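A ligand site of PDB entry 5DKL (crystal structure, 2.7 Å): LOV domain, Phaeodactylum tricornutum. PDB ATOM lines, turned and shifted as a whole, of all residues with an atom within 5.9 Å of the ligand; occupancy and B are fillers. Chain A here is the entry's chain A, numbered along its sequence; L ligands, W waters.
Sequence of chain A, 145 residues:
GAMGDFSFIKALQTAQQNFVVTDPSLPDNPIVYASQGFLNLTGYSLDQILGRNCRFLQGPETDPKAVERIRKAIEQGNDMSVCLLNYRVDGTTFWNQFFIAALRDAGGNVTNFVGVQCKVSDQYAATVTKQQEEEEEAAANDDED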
ATOM      1  N   VAL A  20       3.814 -20.483  -0.736  1.00  0.00           N
ATOM      2  CA  VAL A  20       4.591 -20.544   0.485  1.00  0.00           C
ATOM      3  C   VAL A  20       5.921 -21.151   0.132  1.00  0.00           C
ATOM      4  O   VAL A  20       6.057 -21.833  -0.895  1.00  0.00           O
ATOM      5  CB  VAL A  20       3.936 -21.406   1.563  1.00  0.00           C
ATOM      6  CG1 VAL A  20       2.614 -20.798   2.010  1.00  0.00           C
ATOM      7  CG2 VAL A  20       3.739 -22.813   1.047  1.00  0.00           C
ATOM      8  N   VAL A  21       6.910 -20.894   0.992  1.00  0.00           N
ATOM      9  CA  VAL A  21       8.188 -21.581   0.889  1.00  0.00           C
ATOM     10  C   VAL A  21       8.441 -22.309   2.186  1.00  0.00           C
ATOM     11  O   VAL A  21       8.238 -21.753   3.270  1.00  0.00           O
ATOM     12  CB  VAL A  21       9.323 -20.633   0.620  1.00  0.00           C
ATOM     13  CG1 VAL A  21      10.550 -21.419   0.232  1.00  0.00           C
ATOM     14  CG2 VAL A  21       8.934 -19.662  -0.471  1.00  0.00           C
ATOM     15  N   THR A  22       8.865 -23.566   2.085  1.00  0.00           N
ATOM     16  CA  THR A  22       9.218 -24.335   3.269  1.00  0.00           C
ATOM     17  C   THR A  22      10.711 -24.668   3.294  1.00  0.00           C
ATOM     18  O   THR A  22      11.380 -24.613   2.267  1.00  0.00           O
ATOM     19  CB  THR A  22       8.384 -25.625   3.379  1.00  0.00           C
ATOM     20  OG1 THR A  22       8.852 -26.577   2.427  1.00  0.00           O
ATOM     21  CG2 THR A  22       6.923 -25.356   3.140  1.00  0.00           C
ATOM     22  N   ASP A  28      10.500 -30.890  10.658  1.00  0.00           N
ATOM     23  CA  ASP A  28       9.108 -30.925  10.192  1.00  0.00           C
ATOM     24  C   ASP A  28       8.795 -29.944   9.052  1.00  0.00           C
ATOM     25  O   ASP A  28       7.646 -29.527   8.890  1.00  0.00           O
ATOM     26  CB  ASP A  28       8.155 -30.674  11.349  1.00  0.00           C
ATOM     27  CG  ASP A  28       6.823 -31.391  11.160  1.00  0.00           C
ATOM     28  OD1 ASP A  28       6.794 -32.399  10.433  1.00  0.00           O
ATOM     29  OD2 ASP A  28       5.812 -30.935  11.741  1.00  0.00           O
ATOM     30  N   ASN A  29       9.815 -29.578   8.278  1.00  0.00           N
ATOM     31  CA  ASN A  29       9.626 -28.791   7.053  1.00  0.00           C
ATOM     32  C   ASN A  29       8.704 -27.575   7.200  1.00  0.00           C
ATOM     33  O   ASN A  29       7.711 -27.473   6.531  1.00  0.00           O
ATOM     34  CB  ASN A  29       9.055 -29.708   5.969  1.00  0.00           C
ATOM     35  CG  ASN A  29       9.125 -29.091   4.583  1.00  0.00           C
ATOM     36  OD1 ASN A  29      10.148 -28.502   4.191  1.00  0.00           O
ATOM     37  ND2 ASN A  29       8.025 -29.211   3.838  1.00  0.00           N
ATOM     38  N   PHE A  38      -1.413 -16.041  -0.297  1.00  0.00           N
ATOM     39  CA  PHE A  38      -1.660 -17.109   0.660  1.00  0.00           C
ATOM     40  C   PHE A  38      -2.369 -16.586   1.902  1.00  0.00           C
ATOM     41  O   PHE A  38      -3.282 -17.233   2.417  1.00  0.00           O
ATOM     42  CB  PHE A  38      -0.351 -17.803   1.036  1.00  0.00           C
ATOM     43  CG  PHE A  38      -0.535 -18.952   1.981  1.00  0.00           C
ATOM     44  CD1 PHE A  38      -1.031 -20.154   1.547  1.00  0.00           C
ATOM     45  CD2 PHE A  38      -0.173 -18.826   3.310  1.00  0.00           C
ATOM     46  CE1 PHE A  38      -1.193 -21.211   2.426  1.00  0.00           C
ATOM     47  CE2 PHE A  38      -0.323 -19.887   4.196  1.00  0.00           C
ATOM     48  CZ  PHE A  38      -0.827 -21.079   3.750  1.00  0.00           C
ATOM     49  N   ASN A  53       4.456 -26.422   9.765  1.00  0.00           N
ATOM     50  CA  ASN A  53       4.122 -27.221   8.591  1.00  0.00           C
ATOM     51  C   ASN A  53       2.714 -26.883   8.144  1.00  0.00           C
ATOM     52  O   ASN A  53       1.792 -26.907   8.971  1.00  0.00           O
ATOM     53  CB  ASN A  53       4.229 -28.698   8.906  1.00  0.00           C
ATOM     54  CG  ASN A  53       4.175 -29.556   7.671  1.00  0.00           C
ATOM     55  OD1 ASN A  53       3.120 -29.717   7.054  1.00  0.00           O
ATOM     56  ND2 ASN A  53       5.329 -30.099   7.292  1.00  0.00           N
ATOM     57  N   CYS A  54       2.509 -26.590   6.849  1.00  0.00           N
ATOM     58  CA  CYS A  54       1.187 -26.124   6.432  1.00  0.00           C
ATOM     59  C   CYS A  54       0.117 -27.225   6.496  1.00  0.00           C
ATOM     60  O   CYS A  54      -1.003 -27.013   6.036  1.00  0.00           O
ATOM     61  CB  CYS A  54       1.217 -25.486   5.023  1.00  0.00           C
ATOM     62  SG  CYS A  54       1.561 -26.567   3.619  1.00  0.00           S
ATOM     63  N   ARG A  55       0.436 -28.365   7.109  1.00  0.00           N
ATOM     64  CA  ARG A  55      -0.605 -29.332   7.467  1.00  0.00           C
ATOM     65  C   ARG A  55      -1.576 -28.718   8.487  1.00  0.00           C
ATOM     66  O   ARG A  55      -2.641 -29.279   8.756  1.00  0.00           O
ATOM     67  CB  ARG A  55       0.001 -30.635   8.023  1.00  0.00           C
ATOM     68  CG  ARG A  55       0.255 -30.638   9.533  1.00  0.00           C
ATOM     69  CD  ARG A  55       0.577 -32.042  10.075  1.00  0.00           C
ATOM     70  NE  ARG A  55       1.808 -32.624   9.532  1.00  0.00           N
ATOM     71  CZ  ARG A  55       3.039 -32.223   9.857  1.00  0.00           C
ATOM     72  NH1 ARG A  55       3.212 -31.218  10.712  1.00  0.00           N
ATOM     73  NH2 ARG A  55       4.105 -32.813   9.314  1.00  0.00           N
ATOM     74  N   PHE A  56      -1.230 -27.557   9.051  1.00  0.00           N
ATOM     75  CA  PHE A  56      -2.134 -26.886   9.982  1.00  0.00           C
ATOM     76  C   PHE A  56      -3.424 -26.425   9.302  1.00  0.00           C
ATOM     77  O   PHE A  56      -4.427 -26.139   9.965  1.00  0.00           O
ATOM     78  CB  PHE A  56      -1.435 -25.712  10.669  1.00  0.00           C
ATOM     79  CG  PHE A  56      -1.392 -24.450   9.856  1.00  0.00           C
ATOM     80  CD1 PHE A  56      -2.452 -23.548   9.899  1.00  0.00           C
ATOM     81  CD2 PHE A  56      -0.261 -24.132   9.112  1.00  0.00           C
ATOM     82  CE1 PHE A  56      -2.406 -22.363   9.154  1.00  0.00           C
ATOM     83  CE2 PHE A  56      -0.215 -22.947   8.368  1.00  0.00           C
ATOM     84  CZ  PHE A  56      -1.286 -22.069   8.391  1.00  0.00           C
ATOM     85  N   LEU A  57      -3.392 -26.361   7.970  1.00  0.00           N
ATOM     86  CA  LEU A  57      -4.558 -25.950   7.203  1.00  0.00           C
ATOM     87  C   LEU A  57      -5.565 -27.084   7.134  1.00  0.00           C
ATOM     88  O   LEU A  57      -6.743 -26.878   6.797  1.00  0.00           O
ATOM     89  CB  LEU A  57      -4.138 -25.496   5.810  1.00  0.00           C
ATOM     90  CG  LEU A  57      -3.393 -24.154   5.816  1.00  0.00           C
ATOM     91  CD1 LEU A  57      -2.707 -23.917   4.476  1.00  0.00           C
ATOM     92  CD2 LEU A  57      -4.349 -23.007   6.136  1.00  0.00           C
ATOM     93  N   GLN A  58      -5.096 -28.280   7.499  1.00  0.00           N
ATOM     94  CA  GLN A  58      -5.948 -29.457   7.519  1.00  0.00           C
ATOM     95  C   GLN A  58      -6.846 -29.444   8.749  1.00  0.00           C
ATOM     96  O   GLN A  58      -6.725 -28.565   9.603  1.00  0.00           O
ATOM     97  CB  GLN A  58      -5.105 -30.733   7.482  1.00  0.00           C
ATOM     98  CG  GLN A  58      -4.253 -30.825   6.227  1.00  0.00           C
ATOM     99  CD  GLN A  58      -3.104 -31.807   6.352  1.00  0.00           C
ATOM    100  OE1 GLN A  58      -3.095 -32.689   7.229  1.00  0.00           O
ATOM    101  NE2 GLN A  58      -2.103 -31.658   5.474  1.00  0.00           N
ATOM    102  N   VAL A  67      -3.641 -36.985   2.240  1.00  0.00           N
ATOM    103  CA  VAL A  67      -2.500 -36.506   3.013  1.00  0.00           C
ATOM    104  C   VAL A  67      -1.338 -37.506   2.967  1.00  0.00           C
ATOM    105  O   VAL A  67      -0.185 -37.138   2.745  1.00  0.00           O
ATOM    106  CB  VAL A  67      -2.880 -36.247   4.479  1.00  0.00           C
ATOM    107  CG1 VAL A  67      -1.648 -36.024   5.312  1.00  0.00           C
ATOM    108  CG2 VAL A  67      -3.818 -35.052   4.570  1.00  0.00           C
ATOM    109  N   GLU A  68      -1.671 -38.775   3.185  1.00  0.00           N
ATOM    110  CA  GLU A  68      -0.692 -39.857   3.157  1.00  0.00           C
ATOM    111  C   GLU A  68       0.007 -39.840   1.806  1.00  0.00           C
ATOM    112  O   GLU A  68       1.230 -39.903   1.733  1.00  0.00           O
ATOM    113  CB  GLU A  68      -1.366 -41.200   3.419  1.00  0.00           C
ATOM    114  CG  GLU A  68      -0.439 -42.382   3.723  1.00  0.00           C
ATOM    115  CD  GLU A  68      -1.214 -43.690   3.930  1.00  0.00           C
ATOM    116  OE1 GLU A  68      -2.136 -43.720   4.784  1.00  0.00           O
ATOM    117  OE2 GLU A  68      -0.911 -44.698   3.221  1.00  0.00           O
ATOM    118  N   ILE A  70       0.304 -37.408  -0.508  1.00  0.00           N
ATOM    119  CA  ILE A  70       1.153 -36.261  -0.797  1.00  0.00           C
ATOM    120  C   ILE A  70       2.423 -36.270   0.067  1.00  0.00           C
ATOM    121  O   ILE A  70       3.446 -35.791  -0.389  1.00  0.00           O
ATOM    122  CB  ILE A  70       0.386 -34.911  -0.626  1.00  0.00           C
ATOM    123  CG1 ILE A  70       1.239 -33.736  -1.128  1.00  0.00           C
ATOM    124  CG2 ILE A  70      -0.103 -34.711   0.804  1.00  0.00           C
ATOM    125  CD1 ILE A  70       1.554 -33.794  -2.631  1.00  0.00           C
ATOM    126  N   ARG A  71       2.386 -36.818   1.280  1.00  0.00           N
ATOM    127  CA  ARG A  71       3.620 -36.928   2.061  1.00  0.00           C
ATOM    128  C   ARG A  71       4.564 -37.942   1.417  1.00  0.00           C
ATOM    129  O   ARG A  71       5.785 -37.747   1.392  1.00  0.00           O
ATOM    130  CB  ARG A  71       3.367 -37.351   3.504  1.00  0.00           C
ATOM    131  CG  ARG A  71       4.670 -37.481   4.316  1.00  0.00           C
ATOM    132  CD  ARG A  71       4.547 -38.444   5.502  1.00  0.00           C
ATOM    133  NE  ARG A  71       3.972 -39.720   5.110  1.00  0.00           N
ATOM    134  CZ  ARG A  71       2.731 -40.109   5.429  1.00  0.00           C
ATOM    135  NH1 ARG A  71       1.946 -39.325   6.168  1.00  0.00           N
ATOM    136  NH2 ARG A  71       2.282 -41.289   5.008  1.00  0.00           N
ATOM    137  N   ILE A  74       6.092 -36.151  -1.511  1.00  0.00           N
ATOM    138  CA  ILE A  74       7.168 -35.228  -1.167  1.00  0.00           C
ATOM    139  C   ILE A  74       8.410 -35.945  -0.643  1.00  0.00           C
ATOM    140  O   ILE A  74       9.501 -35.380  -0.619  1.00  0.00           O
ATOM    141  CB  ILE A  74       6.692 -34.219  -0.100  1.00  0.00           C
ATOM    142  CG1 ILE A  74       5.393 -33.571  -0.560  1.00  0.00           C
ATOM    143  CG2 ILE A  74       7.741 -33.146   0.158  1.00  0.00           C
ATOM    144  CD1 ILE A  74       4.608 -32.932   0.552  1.00  0.00           C
ATOM    145  N   LEU A  84      -6.997 -31.007  -1.350  1.00  0.00           N
ATOM    146  CA  LEU A  84      -7.235 -31.308   0.057  1.00  0.00           C
ATOM    147  C   LEU A  84      -8.235 -30.358   0.687  1.00  0.00           C
ATOM    148  O   LEU A  84      -8.263 -29.150   0.370  1.00  0.00           O
ATOM    149  CB  LEU A  84      -5.948 -31.236   0.875  1.00  0.00           C
ATOM    150  CG  LEU A  84      -4.773 -32.195   0.729  1.00  0.00           C
ATOM    151  CD1 LEU A  84      -3.745 -31.846   1.786  1.00  0.00           C
ATOM    152  CD2 LEU A  84      -5.231 -33.603   0.907  1.00  0.00           C
ATOM    153  N   LEU A  85      -9.042 -30.883   1.594  1.00  0.00           N
ATOM    154  CA  LEU A  85      -9.940 -30.032   2.343  1.00  0.00           C
ATOM    155  C   LEU A  85      -9.072 -29.240   3.335  1.00  0.00           C
ATOM    156  O   LEU A  85      -8.192 -29.795   3.997  1.00  0.00           O
ATOM    157  CB  LEU A  85     -10.999 -30.873   3.053  1.00  0.00           C
ATOM    158  CG  LEU A  85     -12.253 -30.162   3.539  1.00  0.00           C
ATOM    159  CD1 LEU A  85     -12.581 -28.978   2.653  1.00  0.00           C
ATOM    160  CD2 LEU A  85     -13.402 -31.150   3.537  1.00  0.00           C
ATOM    161  N   ASN A  86      -9.284 -27.935   3.380  1.00  0.00           N
ATOM    162  CA  ASN A  86      -8.448 -27.044   4.148  1.00  0.00           C
ATOM    163  C   ASN A  86      -9.344 -26.075   4.883  1.00  0.00           C
ATOM    164  O   ASN A  86     -10.420 -25.721   4.385  1.00  0.00           O
ATOM    165  CB  ASN A  86      -7.448 -26.289   3.251  1.00  0.00           C
ATOM    166  CG  ASN A  86      -6.112 -27.013   3.132  1.00  0.00           C
ATOM    167  OD1 ASN A  86      -5.090 -26.425   2.740  1.00  0.00           O
ATOM    168  ND2 ASN A  86      -6.105 -28.285   3.476  1.00  0.00           N
ATOM    169  N   ASN A  96      -8.423 -27.058  -1.715  1.00  0.00           N
ATOM    170  CA  ASN A  96      -7.135 -26.493  -2.065  1.00  0.00           C
ATOM    171  C   ASN A  96      -6.386 -27.429  -3.001  1.00  0.00           C
ATOM    172  O   ASN A  96      -5.873 -28.475  -2.579  1.00  0.00           O
ATOM    173  CB  ASN A  96      -6.327 -26.212  -0.790  1.00  0.00           C
ATOM    174  CG  ASN A  96      -5.028 -25.463  -1.066  1.00  0.00           C
ATOM    175  OD1 ASN A  96      -4.607 -25.323  -2.223  1.00  0.00           O
ATOM    176  ND2 ASN A  96      -4.377 -24.985   0.004  1.00  0.00           N
ATOM    177  N   PHE A  98      -3.090 -27.772  -4.841  1.00  0.00           N
ATOM    178  CA  PHE A  98      -1.800 -27.094  -4.821  1.00  0.00           C
ATOM    179  C   PHE A  98      -0.671 -27.959  -5.365  1.00  0.00           C
ATOM    180  O   PHE A  98      -0.724 -29.193  -5.324  1.00  0.00           O
ATOM    181  CB  PHE A  98      -1.456 -26.603  -3.394  1.00  0.00           C
ATOM    182  CG  PHE A  98      -1.323 -27.680  -2.356  1.00  0.00           C
ATOM    183  CD1 PHE A  98      -0.095 -28.307  -2.123  1.00  0.00           C
ATOM    184  CD2 PHE A  98      -2.417 -28.056  -1.584  1.00  0.00           C
ATOM    185  CE1 PHE A  98       0.038 -29.303  -1.145  1.00  0.00           C
ATOM    186  CE2 PHE A  98      -2.300 -29.056  -0.607  1.00  0.00           C
ATOM    187  CZ  PHE A  98      -1.068 -29.677  -0.379  1.00  0.00           C
ATOM    188  N   ILE A 100       3.573 -28.575  -5.594  1.00  0.00           N
ATOM    189  CA  ILE A 100       4.793 -28.410  -4.839  1.00  0.00           C
ATOM    190  C   ILE A 100       5.981 -28.699  -5.731  1.00  0.00           C
ATOM    191  O   ILE A 100       6.020 -29.738  -6.386  1.00  0.00           O
ATOM    192  CB  ILE A 100       4.821 -29.345  -3.605  1.00  0.00           C
ATOM    193  CG1 ILE A 100       3.712 -28.985  -2.616  1.00  0.00           C
ATOM    194  CG2 ILE A 100       6.169 -29.300  -2.896  1.00  0.00           C
ATOM    195  CD1 ILE A 100       3.336 -30.120  -1.702  1.00  0.00           C
ATOM    196  N   ALA A 101       6.933 -27.781  -5.758  1.00  0.00           N
ATOM    197  CA  ALA A 101       8.204 -27.990  -6.450  1.00  0.00           C
ATOM    198  C   ALA A 101       9.402 -27.823  -5.498  1.00  0.00           C
ATOM    199  O   ALA A 101       9.391 -26.974  -4.592  1.00  0.00           O
ATOM    200  CB  ALA A 101       8.316 -27.035  -7.601  1.00  0.00           C
ATOM    201  N   PHE A 113      11.221 -26.030  -0.553  1.00  0.00           N
ATOM    202  CA  PHE A 113      10.058 -26.320  -1.360  1.00  0.00           C
ATOM    203  C   PHE A 113       9.246 -25.072  -1.563  1.00  0.00           C
ATOM    204  O   PHE A 113       9.182 -24.222  -0.663  1.00  0.00           O
ATOM    205  CB  PHE A 113       9.194 -27.405  -0.706  1.00  0.00           C
ATOM    206  CG  PHE A 113       9.776 -28.778  -0.786  1.00  0.00           C
ATOM    207  CD1 PHE A 113       9.610 -29.558  -1.928  1.00  0.00           C
ATOM    208  CD2 PHE A 113      10.513 -29.291   0.275  1.00  0.00           C
ATOM    209  CE1 PHE A 113      10.153 -30.823  -1.996  1.00  0.00           C
ATOM    210  CE2 PHE A 113      11.056 -30.555   0.207  1.00  0.00           C
ATOM    211  CZ  PHE A 113      10.874 -31.327  -0.919  1.00  0.00           C
ATOM    212  N   VAL A 114       8.629 -24.943  -2.733  1.00  0.00           N
ATOM    213  CA  VAL A 114       7.694 -23.864  -2.975  1.00  0.00           C
ATOM    214  C   VAL A 114       6.361 -24.494  -3.325  1.00  0.00           C
ATOM    215  O   VAL A 114       6.310 -25.526  -3.992  1.00  0.00           O
ATOM    216  CB  VAL A 114       8.168 -22.937  -4.101  1.00  0.00           C
ATOM    217  CG1 VAL A 114       7.300 -21.682  -4.163  1.00  0.00           C
ATOM    218  CG2 VAL A 114       9.614 -22.569  -3.875  1.00  0.00           C
ATOM    219  N   GLY A 115       5.276 -23.887  -2.866  1.00  0.00           N
ATOM    220  CA  GLY A 115       3.969 -24.452  -3.098  1.00  0.00           C
ATOM    221  C   GLY A 115       2.983 -23.379  -3.495  1.00  0.00           C
ATOM    222  O   GLY A 115       2.737 -22.445  -2.725  1.00  0.00           O
ATOM    223  N   GLN A 117      -0.869 -22.414  -4.263  1.00  0.00           N
ATOM    224  CA  GLN A 117      -2.181 -22.900  -3.835  1.00  0.00           C
ATOM    225  C   GLN A 117      -3.290 -22.319  -4.685  1.00  0.00           C
ATOM    226  O   GLN A 117      -3.300 -21.118  -4.959  1.00  0.00           O
ATOM    227  CB  GLN A 117      -2.464 -22.556  -2.365  1.00  0.00           C
ATOM    228  CG  GLN A 117      -1.655 -23.303  -1.356  1.00  0.00           C
ATOM    229  CD  GLN A 117      -0.233 -22.792  -1.240  1.00  0.00           C
ATOM    230  OE1 GLN A 117       0.686 -23.558  -0.928  1.00  0.00           O
ATOM    231  NE2 GLN A 117      -0.038 -21.490  -1.492  1.00  0.00           N
HETATM  232  N1  LIG L   1      -0.782 -29.175   3.016  1.00  0.00           N
HETATM  233  C1  LIG L   1      -2.007 -28.568   3.062  1.00  0.00           C
HETATM  234  O1  LIG L   1      -2.965 -28.988   3.713  1.00  0.00           O
HETATM  235  N2  LIG L   1      -2.193 -27.345   2.373  1.00  0.00           N
HETATM  236  C2  LIG L   1      -1.193 -26.647   1.760  1.00  0.00           C
HETATM  237  O2  LIG L   1      -1.384 -25.667   1.070  1.00  0.00           O
HETATM  238  C3  LIG L   1       0.242 -27.084   2.161  1.00  0.00           C
HETATM  239  N3  LIG L   1       0.917 -26.871   0.924  1.00  0.00           N
HETATM  240  C4  LIG L   1       2.245 -27.316   0.983  1.00  0.00           C
HETATM  241  C5  LIG L   1       3.291 -26.562   0.492  1.00  0.00           C
HETATM  242  C6  LIG L   1       4.582 -27.075   0.454  1.00  0.00           C
HETATM  243  C7  LIG L   1       5.665 -26.286  -0.246  1.00  0.00           C
HETATM  244  C8  LIG L   1       4.833 -28.326   1.056  1.00  0.00           C
HETATM  245  C9  LIG L   1       6.223 -28.931   1.037  1.00  0.00           C
HETATM  246  C10 LIG L   1       3.794 -29.036   1.658  1.00  0.00           C
HETATM  247  C11 LIG L   1       2.490 -28.583   1.558  1.00  0.00           C
HETATM  248  N4  LIG L   1       1.425 -29.204   2.248  1.00  0.00           N
HETATM  249  C12 LIG L   1       0.229 -28.587   2.384  1.00  0.00           C
HETATM  250  C13 LIG L   1       1.587 -30.626   2.729  1.00  0.00           C
HETATM  251  C14 LIG L   1       1.887 -30.714   4.226  1.00  0.00           C
HETATM  252  O3  LIG L   1       2.916 -29.829   4.627  1.00  0.00           O
HETATM  253  C15 LIG L   1       2.275 -32.137   4.601  1.00  0.00           C
HETATM  254  O4  LIG L   1       3.404 -32.500   3.837  1.00  0.00           O
HETATM  255  C16 LIG L   1       1.103 -33.076   4.356  1.00  0.00           C
HETATM  256  O5  LIG L   1       0.105 -32.850   5.340  1.00  0.00           O
HETATM  257  C17 LIG L   1       1.480 -34.553   4.392  1.00  0.00           C
HETATM  258  O6  LIG L   1       2.461 -34.809   5.359  1.00  0.00           O
HETATM  259  P1  LIG L   1       2.089 -35.218   6.864  1.00  0.00           P
HETATM  260  O7  LIG L   1       1.700 -36.679   6.890  1.00  0.00           O
HETATM  261  O8  LIG L   1       3.351 -35.020   7.692  1.00  0.00           O
HETATM  262  O9  LIG L   1       0.965 -34.350   7.417  1.00  0.00           O
HETATM  263  O   HOH W   1       5.770 -31.300   4.650  1.00  0.00           O
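SG of Cys 54 is bonded to C3 of the ligand (2.0 Å). The side-chain amide oxygen (OD1) of Asn 53 lies within hydrogen-bond range of an oxygen (O3) of the ligand. The side-chain amide nitrogen of Gln 58 is in hydrogen-bond range of an oxygen (O5) of the ligand, at 2.5 Å. NH1 of Arg 71 is in salt-bridge range of O7 of the ligand (2.8 Å). NH2 of Arg 55 lies within salt-bridge range of O8 of the ligand (2.8 Å). The side-chain amide oxygen (OD1) of Asn 86 sits at hydrogen-bond distance from a nitrogen (N2) of the ligand, at 3.1 Å. ND2 of Asn 96 sits at hydrogen-bond distance from O2 of the ligand, at 3.2 Å.
Val 20 touches the ligand (CG2 to C5, 3.8 Å). CG2 of Thr 22 touches C7 of the ligand (3.7 Å). Asn 29 touches the ligand. Val 67 touches the ligand (O to C17, 3.5 Å). Ile 70 touches the ligand. Ile 74 touches the ligand (CD1 to O4, 3.5 Å). Leu 84 touches the ligand. Phe 98 touches the ligand (CZ to C12, 3.2 Å). Ile 100 touches the ligand (CD1 to C10, 3.6 Å). CB of Phe 113 touches C7 of the ligand, at 3.7 Å. Val 114 touches the ligand. N of Gly 115 touches C7 of the ligand (3.6 Å). CG of Gln 117 touches O2 of the ligand (3.4 Å). Of the 28 residues printed, 20 come within 4 Å of the ligand.
Water W1 lies within hydrogen-bond range of an oxygen (O4) of the ligand (2.8 Å), the side-chain amide nitrogen (ND2) of Asn 53 (2.9 Å) and the side-chain amide nitrogen (ND2) of Asn 29 (3.2 Å).
The side-chain amide oxygen of Asn 53 lies close to the backbone NH of Arg 55 (3.0 Å). O of Asp 28 is in hydrogen-bond range of ND2 of Asn 53 (2.9 Å). NH1 of Arg 55 is in salt-bridge range of OD2 of Asp 28 (2.8 Å). OD1 of Asn 86 lies within hydrogen-bond range of ND2 of Asn 96 (3.2 Å). N of Asn 96 is in hydrogen-bond range of O of Leu 84 (3.0 Å). The backbone NH of Gly 115 sits at hydrogen-bond distance from the backbone carbonyl oxygen of Val 20, 3.0 Å away. The backbone carbonyl oxygen (O) of Ala 101 lies within hydrogen-bond range of the backbone NH (N) of Val 114. O of Phe 113 lies within hydrogen-bond range of N of Thr 22 (2.8 Å).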
